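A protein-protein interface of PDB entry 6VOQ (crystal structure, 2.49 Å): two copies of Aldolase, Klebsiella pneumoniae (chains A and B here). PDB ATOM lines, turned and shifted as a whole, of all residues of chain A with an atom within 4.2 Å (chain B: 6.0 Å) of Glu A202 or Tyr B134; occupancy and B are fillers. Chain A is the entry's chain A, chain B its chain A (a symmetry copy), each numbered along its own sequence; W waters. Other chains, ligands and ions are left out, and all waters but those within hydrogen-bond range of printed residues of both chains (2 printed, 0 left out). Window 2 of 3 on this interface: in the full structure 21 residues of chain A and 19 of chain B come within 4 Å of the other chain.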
ATOM      1  N   PRO A 120      10.707 -18.128 -11.507  1.00  0.00           N
ATOM      2  CA  PRO A 120      11.105 -19.475 -11.079  1.00  0.00           C
ATOM      3  C   PRO A 120      12.475 -19.565 -10.427  1.00  0.00           C
ATOM      4  O   PRO A 120      12.752 -20.564  -9.752  1.00  0.00           O
ATOM      5  CB  PRO A 120      11.084 -20.269 -12.393  1.00  0.00           C
ATOM      6  CG  PRO A 120      11.426 -19.263 -13.412  1.00  0.00           C
ATOM      7  CD  PRO A 120      10.790 -17.970 -12.969  1.00  0.00           C
ATOM      8  N   ARG A 196       0.919 -11.824 -11.728  1.00  0.00           N
ATOM      9  CA  ARG A 196       0.720 -13.224 -12.113  1.00  0.00           C
ATOM     10  C   ARG A 196       1.694 -14.085 -11.309  1.00  0.00           C
ATOM     11  O   ARG A 196       2.782 -14.439 -11.767  1.00  0.00           O
ATOM     12  CB  ARG A 196       0.943 -13.399 -13.616  1.00  0.00           C
ATOM     13  CG  ARG A 196      -0.040 -14.326 -14.340  1.00  0.00           C
ATOM     14  CD  ARG A 196       0.059 -15.772 -13.880  1.00  0.00           C
ATOM     15  NE  ARG A 196       1.325 -16.393 -14.252  1.00  0.00           N
ATOM     16  CZ  ARG A 196       1.642 -17.661 -13.998  1.00  0.00           C
ATOM     17  NH1 ARG A 196       0.792 -18.462 -13.370  1.00  0.00           N
ATOM     18  NH2 ARG A 196       2.820 -18.129 -14.362  1.00  0.00           N
ATOM     19  N   LEU A 198       3.324 -17.377  -9.467  1.00  0.00           N
ATOM     20  CA  LEU A 198       3.438 -18.770  -9.871  1.00  0.00           C
ATOM     21  C   LEU A 198       2.441 -19.603  -9.079  1.00  0.00           C
ATOM     22  O   LEU A 198       2.318 -19.443  -7.859  1.00  0.00           O
ATOM     23  CB  LEU A 198       4.855 -19.283  -9.657  1.00  0.00           C
ATOM     24  CG  LEU A 198       5.963 -18.699 -10.539  1.00  0.00           C
ATOM     25  CD1 LEU A 198       7.214 -19.584 -10.489  1.00  0.00           C
ATOM     26  CD2 LEU A 198       5.483 -18.509 -11.963  1.00  0.00           C
ATOM     27  N   THR A 199       1.708 -20.477  -9.775  1.00  0.00           N
ATOM     28  CA  THR A 199       0.738 -21.335  -9.114  1.00  0.00           C
ATOM     29  C   THR A 199       1.445 -22.306  -8.183  1.00  0.00           C
ATOM     30  O   THR A 199       2.665 -22.482  -8.235  1.00  0.00           O
ATOM     31  CB  THR A 199      -0.094 -22.109 -10.134  1.00  0.00           C
ATOM     32  OG1 THR A 199       0.728 -23.084 -10.801  1.00  0.00           O
ATOM     33  CG2 THR A 199      -0.705 -21.159 -11.153  1.00  0.00           C
ATOM     34  N   ALA A 200       0.659 -22.953  -7.325  1.00  0.00           N
ATOM     35  CA  ALA A 200       1.240 -23.931  -6.415  1.00  0.00           C
ATOM     36  C   ALA A 200       1.905 -25.069  -7.183  1.00  0.00           C
ATOM     37  O   ALA A 200       2.971 -25.551  -6.786  1.00  0.00           O
ATOM     38  CB  ALA A 200       0.176 -24.468  -5.459  1.00  0.00           C
ATOM     39  N   ASP A 201       1.300 -25.510  -8.289  1.00  0.00           N
ATOM     40  CA  ASP A 201       1.912 -26.587  -9.066  1.00  0.00           C
ATOM     41  C   ASP A 201       3.161 -26.099  -9.777  1.00  0.00           C
ATOM     42  O   ASP A 201       4.140 -26.843  -9.907  1.00  0.00           O
ATOM     43  CB  ASP A 201       0.914 -27.163 -10.070  1.00  0.00           C
ATOM     44  CG  ASP A 201      -0.416 -27.500  -9.427  1.00  0.00           C
ATOM     45  OD1 ASP A 201      -1.215 -26.560  -9.191  1.00  0.00           O
ATOM     46  OD2 ASP A 201      -0.657 -28.695  -9.149  1.00  0.00           O
ATOM     47  N   GLU A 202       3.149 -24.846 -10.236  1.00  0.00           N
ATOM     48  CA  GLU A 202       4.336 -24.280 -10.866  1.00  0.00           C
ATOM     49  C   GLU A 202       5.508 -24.158  -9.888  1.00  0.00           C
ATOM     50  O   GLU A 202       6.668 -24.219 -10.310  1.00  0.00           O
ATOM     51  CB  GLU A 202       3.987 -22.929 -11.481  1.00  0.00           C
ATOM     52  CG  GLU A 202       3.188 -23.062 -12.762  1.00  0.00           C
ATOM     53  CD  GLU A 202       2.559 -21.758 -13.209  1.00  0.00           C
ATOM     54  OE1 GLU A 202       2.155 -21.676 -14.389  1.00  0.00           O
ATOM     55  OE2 GLU A 202       2.473 -20.820 -12.387  1.00  0.00           O
ATOM     56  N   VAL A 203       5.237 -24.001  -8.590  1.00  0.00           N
ATOM     57  CA  VAL A 203       6.323 -23.915  -7.618  1.00  0.00           C
ATOM     58  C   VAL A 203       6.860 -25.298  -7.279  1.00  0.00           C
ATOM     59  O   VAL A 203       8.060 -25.470  -7.046  1.00  0.00           O
ATOM     60  CB  VAL A 203       5.859 -23.169  -6.355  1.00  0.00           C
ATOM     61  CG1 VAL A 203       6.993 -23.102  -5.347  1.00  0.00           C
ATOM     62  CG2 VAL A 203       5.354 -21.758  -6.705  1.00  0.00           C
ATOM     63  N   LYS A 204       5.987 -26.304  -7.231  1.00  0.00           N
ATOM     64  CA  LYS A 204       6.444 -27.649  -6.929  1.00  0.00           C
ATOM     65  C   LYS A 204       7.284 -28.226  -8.059  1.00  0.00           C
ATOM     66  O   LYS A 204       8.161 -29.056  -7.801  1.00  0.00           O
ATOM     67  CB  LYS A 204       5.244 -28.553  -6.624  1.00  0.00           C
ATOM     68  CG  LYS A 204       5.620 -29.881  -5.981  1.00  0.00           C
ATOM     69  CD  LYS A 204       4.612 -30.305  -4.916  1.00  0.00           C
ATOM     70  CE  LYS A 204       4.673 -29.400  -3.682  1.00  0.00           C
ATOM     71  NZ  LYS A 204       5.486 -30.010  -2.584  1.00  0.00           N
ATOM     72  N   GLU A 205       7.053 -27.788  -9.302  1.00  0.00           N
ATOM     73  CA  GLU A 205       7.841 -28.276 -10.426  1.00  0.00           C
ATOM     74  C   GLU A 205       9.315 -27.917 -10.306  1.00  0.00           C
ATOM     75  O   GLU A 205      10.150 -28.564 -10.949  1.00  0.00           O
ATOM     76  CB  GLU A 205       7.322 -27.699 -11.740  1.00  0.00           C
ATOM     77  CG  GLU A 205       5.991 -28.207 -12.198  1.00  0.00           C
ATOM     78  CD  GLU A 205       5.279 -27.198 -13.081  1.00  0.00           C
ATOM     79  OE1 GLU A 205       4.026 -27.177 -13.062  1.00  0.00           O
ATOM     80  OE2 GLU A 205       5.972 -26.424 -13.784  1.00  0.00           O
ATOM     81  N   LEU A 206       9.649 -26.896  -9.516  1.00  0.00           N
ATOM     82  CA  LEU A 206      10.982 -26.311  -9.496  1.00  0.00           C
ATOM     83  C   LEU A 206      11.829 -26.805  -8.330  1.00  0.00           C
ATOM     84  O   LEU A 206      12.653 -26.056  -7.806  1.00  0.00           O
ATOM     85  CB  LEU A 206      10.882 -24.786  -9.462  1.00  0.00           C
ATOM     86  CG  LEU A 206       9.932 -24.157 -10.477  1.00  0.00           C
ATOM     87  CD1 LEU A 206       9.595 -22.730 -10.077  1.00  0.00           C
ATOM     88  CD2 LEU A 206      10.558 -24.185 -11.854  1.00  0.00           C
ATOM     89  N   VAL B 132       4.578 -14.411 -24.413  1.00  0.00           N
ATOM     90  CA  VAL B 132       4.528 -15.864 -24.368  1.00  0.00           C
ATOM     91  C   VAL B 132       4.086 -16.240 -22.964  1.00  0.00           C
ATOM     92  O   VAL B 132       4.611 -15.678 -21.993  1.00  0.00           O
ATOM     93  CB  VAL B 132       5.885 -16.491 -24.718  1.00  0.00           C
ATOM     94  CG1 VAL B 132       5.840 -17.990 -24.462  1.00  0.00           C
ATOM     95  CG2 VAL B 132       6.263 -16.166 -26.163  1.00  0.00           C
ATOM     96  N   PRO B 133       3.113 -17.139 -22.808  1.00  0.00           N
ATOM     97  CA  PRO B 133       2.721 -17.574 -21.466  1.00  0.00           C
ATOM     98  C   PRO B 133       3.901 -18.137 -20.692  1.00  0.00           C
ATOM     99  O   PRO B 133       4.926 -18.536 -21.257  1.00  0.00           O
ATOM    100  CB  PRO B 133       1.659 -18.646 -21.734  1.00  0.00           C
ATOM    101  CG  PRO B 133       1.113 -18.306 -23.073  1.00  0.00           C
ATOM    102  CD  PRO B 133       2.263 -17.735 -23.851  1.00  0.00           C
ATOM    103  N   TYR B 134       3.766 -18.123 -19.368  1.00  0.00           N
ATOM    104  CA  TYR B 134       4.797 -18.708 -18.528  1.00  0.00           C
ATOM    105  C   TYR B 134       4.755 -20.223 -18.639  1.00  0.00           C
ATOM    106  O   TYR B 134       3.683 -20.837 -18.606  1.00  0.00           O
ATOM    107  CB  TYR B 134       4.630 -18.316 -17.061  1.00  0.00           C
ATOM    108  CG  TYR B 134       5.525 -19.171 -16.198  1.00  0.00           C
ATOM    109  CD1 TYR B 134       6.891 -18.921 -16.136  1.00  0.00           C
ATOM    110  CD2 TYR B 134       5.029 -20.278 -15.515  1.00  0.00           C
ATOM    111  CE1 TYR B 134       7.736 -19.720 -15.388  1.00  0.00           C
ATOM    112  CE2 TYR B 134       5.871 -21.093 -14.769  1.00  0.00           C
ATOM    113  CZ  TYR B 134       7.226 -20.797 -14.703  1.00  0.00           C
ATOM    114  OH  TYR B 134       8.080 -21.586 -13.965  1.00  0.00           O
ATOM    115  N   TYR B 135       5.938 -20.819 -18.756  1.00  0.00           N
ATOM    116  CA  TYR B 135       6.120 -22.261 -18.710  1.00  0.00           C
ATOM    117  C   TYR B 135       7.394 -22.554 -17.940  1.00  0.00           C
ATOM    118  O   TYR B 135       8.339 -21.766 -17.958  1.00  0.00           O
ATOM    119  CB  TYR B 135       6.235 -22.881 -20.111  1.00  0.00           C
ATOM    120  CG  TYR B 135       5.031 -22.687 -20.998  1.00  0.00           C
ATOM    121  CD1 TYR B 135       3.834 -23.337 -20.726  1.00  0.00           C
ATOM    122  CD2 TYR B 135       5.102 -21.875 -22.132  1.00  0.00           C
ATOM    123  CE1 TYR B 135       2.730 -23.173 -21.548  1.00  0.00           C
ATOM    124  CE2 TYR B 135       4.000 -21.704 -22.961  1.00  0.00           C
ATOM    125  CZ  TYR B 135       2.818 -22.356 -22.663  1.00  0.00           C
ATOM    126  OH  TYR B 135       1.720 -22.200 -23.478  1.00  0.00           O
ATOM    127  N   ARG B 136       7.414 -23.708 -17.287  1.00  0.00           N
ATOM    128  CA  ARG B 136       8.605 -24.167 -16.589  1.00  0.00           C
ATOM    129  C   ARG B 136       9.835 -23.988 -17.477  1.00  0.00           C
ATOM    130  O   ARG B 136       9.780 -24.288 -18.677  1.00  0.00           O
ATOM    131  CB  ARG B 136       8.446 -25.642 -16.198  1.00  0.00           C
ATOM    132  CG  ARG B 136       9.412 -26.111 -15.144  1.00  0.00           C
ATOM    133  CD  ARG B 136       9.946 -27.471 -15.491  1.00  0.00           C
ATOM    134  NE  ARG B 136      10.380 -28.215 -14.313  1.00  0.00           N
ATOM    135  CZ  ARG B 136      11.542 -28.022 -13.698  1.00  0.00           C
ATOM    136  NH1 ARG B 136      12.392 -27.101 -14.142  1.00  0.00           N
ATOM    137  NH2 ARG B 136      11.856 -28.753 -12.636  1.00  0.00           N
ATOM    138  N   PRO B 137      10.936 -23.462 -16.949  1.00  0.00           N
ATOM    139  CA  PRO B 137      12.156 -23.338 -17.755  1.00  0.00           C
ATOM    140  C   PRO B 137      12.564 -24.674 -18.362  1.00  0.00           C
ATOM    141  O   PRO B 137      12.582 -25.711 -17.685  1.00  0.00           O
ATOM    142  CB  PRO B 137      13.189 -22.828 -16.749  1.00  0.00           C
ATOM    143  CG  PRO B 137      12.364 -22.058 -15.756  1.00  0.00           C
ATOM    144  CD  PRO B 137      11.072 -22.814 -15.634  1.00  0.00           C
ATOM    145  N   LEU B 158       8.623 -13.146 -22.618  1.00  0.00           N
ATOM    146  CA  LEU B 158       8.291 -14.390 -21.936  1.00  0.00           C
ATOM    147  C   LEU B 158       7.728 -14.058 -20.561  1.00  0.00           C
ATOM    148  O   LEU B 158       8.431 -13.486 -19.722  1.00  0.00           O
ATOM    149  CB  LEU B 158       9.522 -15.281 -21.798  1.00  0.00           C
ATOM    150  CG  LEU B 158      10.353 -15.580 -23.037  1.00  0.00           C
ATOM    151  CD1 LEU B 158      11.442 -16.562 -22.651  1.00  0.00           C
ATOM    152  CD2 LEU B 158       9.503 -16.150 -24.146  1.00  0.00           C
ATOM    153  N   ALA B 159       6.458 -14.384 -20.344  1.00  0.00           N
ATOM    154  CA  ALA B 159       5.806 -14.048 -19.088  1.00  0.00           C
ATOM    155  C   ALA B 159       6.570 -14.654 -17.916  1.00  0.00           C
ATOM    156  O   ALA B 159       7.121 -15.751 -18.022  1.00  0.00           O
ATOM    157  CB  ALA B 159       4.363 -14.543 -19.104  1.00  0.00           C
ATOM    158  N   ASN B 160       6.617 -13.918 -16.803  1.00  0.00           N
ATOM    159  CA  ASN B 160       7.313 -14.357 -15.589  1.00  0.00           C
ATOM    160  C   ASN B 160       8.754 -14.763 -15.880  1.00  0.00           C
ATOM    161  O   ASN B 160       9.265 -15.749 -15.347  1.00  0.00           O
ATOM    162  CB  ASN B 160       6.579 -15.510 -14.908  1.00  0.00           C
ATOM    163  CG  ASN B 160       5.162 -15.174 -14.563  1.00  0.00           C
ATOM    164  OD1 ASN B 160       4.232 -15.497 -15.308  1.00  0.00           O
ATOM    165  ND2 ASN B 160       4.977 -14.525 -13.425  1.00  0.00           N
ATOM    166  N   HIS B 161       9.421 -13.999 -16.736  1.00  0.00           N
ATOM    167  CA  HIS B 161      10.728 -14.424 -17.201  1.00  0.00           C
ATOM    168  C   HIS B 161      11.562 -13.246 -17.674  1.00  0.00           C
ATOM    169  O   HIS B 161      12.453 -12.789 -16.949  1.00  0.00           O
ATOM    170  CB  HIS B 161      10.565 -15.446 -18.317  1.00  0.00           C
ATOM    171  CG  HIS B 161      11.840 -16.128 -18.699  1.00  0.00           C
ATOM    172  ND1 HIS B 161      11.864 -17.311 -19.403  1.00  0.00           N
ATOM    173  CD2 HIS B 161      13.130 -15.797 -18.471  1.00  0.00           C
ATOM    174  CE1 HIS B 161      13.117 -17.677 -19.596  1.00  0.00           C
ATOM    175  NE2 HIS B 161      13.905 -16.775 -19.039  1.00  0.00           N
HETATM  176  O   HOH W   1       7.106 -23.946 -13.009  1.00  0.00           O
HETATM  177  O   HOH W   2      12.952 -29.826 -10.247  1.00  0.00           O
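Among the printed residues, pairs that only touch across the chains: Arg A196 with Tyr B134, Glu A202 with Tyr B134, Pro A120 with Asn B160, Pro A120 with Tyr B134, Pro A120 with Pro B137, Leu A198 with Tyr B134 and Leu A206 with Arg B136.
No position is printed for both chains. Of the 9 pairs that touch across the chains among the printed residues, none has its exchanged pair printed and touching as well.
OE2 of Glu A202 is in hydrogen-bond range of N of Thr A199, at 2.7 Å. The guanidinium group (NH1) of Arg A196 lies within salt-bridge range of the side-chain carboxylate (OE2) of Glu A202, at 3.1 Å.
Water W1 lies within hydrogen-bond range of OH of Tyr B134 (2.7 Å), O of Glu A202 (2.7 Å) and OE2 of Glu A205 (2.8 Å). Water W2 lies within hydrogen-bond range of the guanidinium group of Arg B136 (2.8 Å) and the backbone carbonyl oxygen of Glu A205 (3.2 Å).
Printed residues of chain B within 4 Å of Pro A120: Tyr B134 (3.6 Å), Pro B137 (3.8 Å) and Asn B160 (3.6 Å). Glu A202 touches one residue of chain B. Printed residues of chain B within 4 Å of Glu A205: Arg B136 (2.4 Å). Of the printed residues of chain B, Leu A206 touches Arg B136. Tyr B134 touches four residues of chain A. Tyr B135 touches none of the printed residues of chain A. Of the printed residues of chain A, Arg B136 touches Glu A205 (2.4 Å) and Leu A206 (3.98 Å). Printed residues of chain A within 4 Å of Pro B137: Pro A120. Ala B159 touches none of the printed residues of chain A. The nearest residue of chain B that does not touch Glu A202 is Tyr B135 (5.8 Å). The nearest printed residue of chain A that does not touch Asn B160 is Leu A198 (4.2 Å).
O of Arg A196 sits at hydrogen-bond distance from ND2 of Asn B160 (2.8 Å). The backbone carbonyl oxygen (O) of Glu A205 is in hydrogen-bond range of the guanidinium group (NH2) of Arg B136 (2.4 Å).
Of the 10 printed residues of chain B, 4 touch a printed residue of chain A. Of the 11 printed residues of chain A, 6 touch a printed residue of chain B. Printed residues of chain A that touch a printed residue of chain B: Pro A120, Arg A196, Leu A198, Glu A202, Glu A205 and Leu A206. Among the printed residues, 9 pairs touch across the chains.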
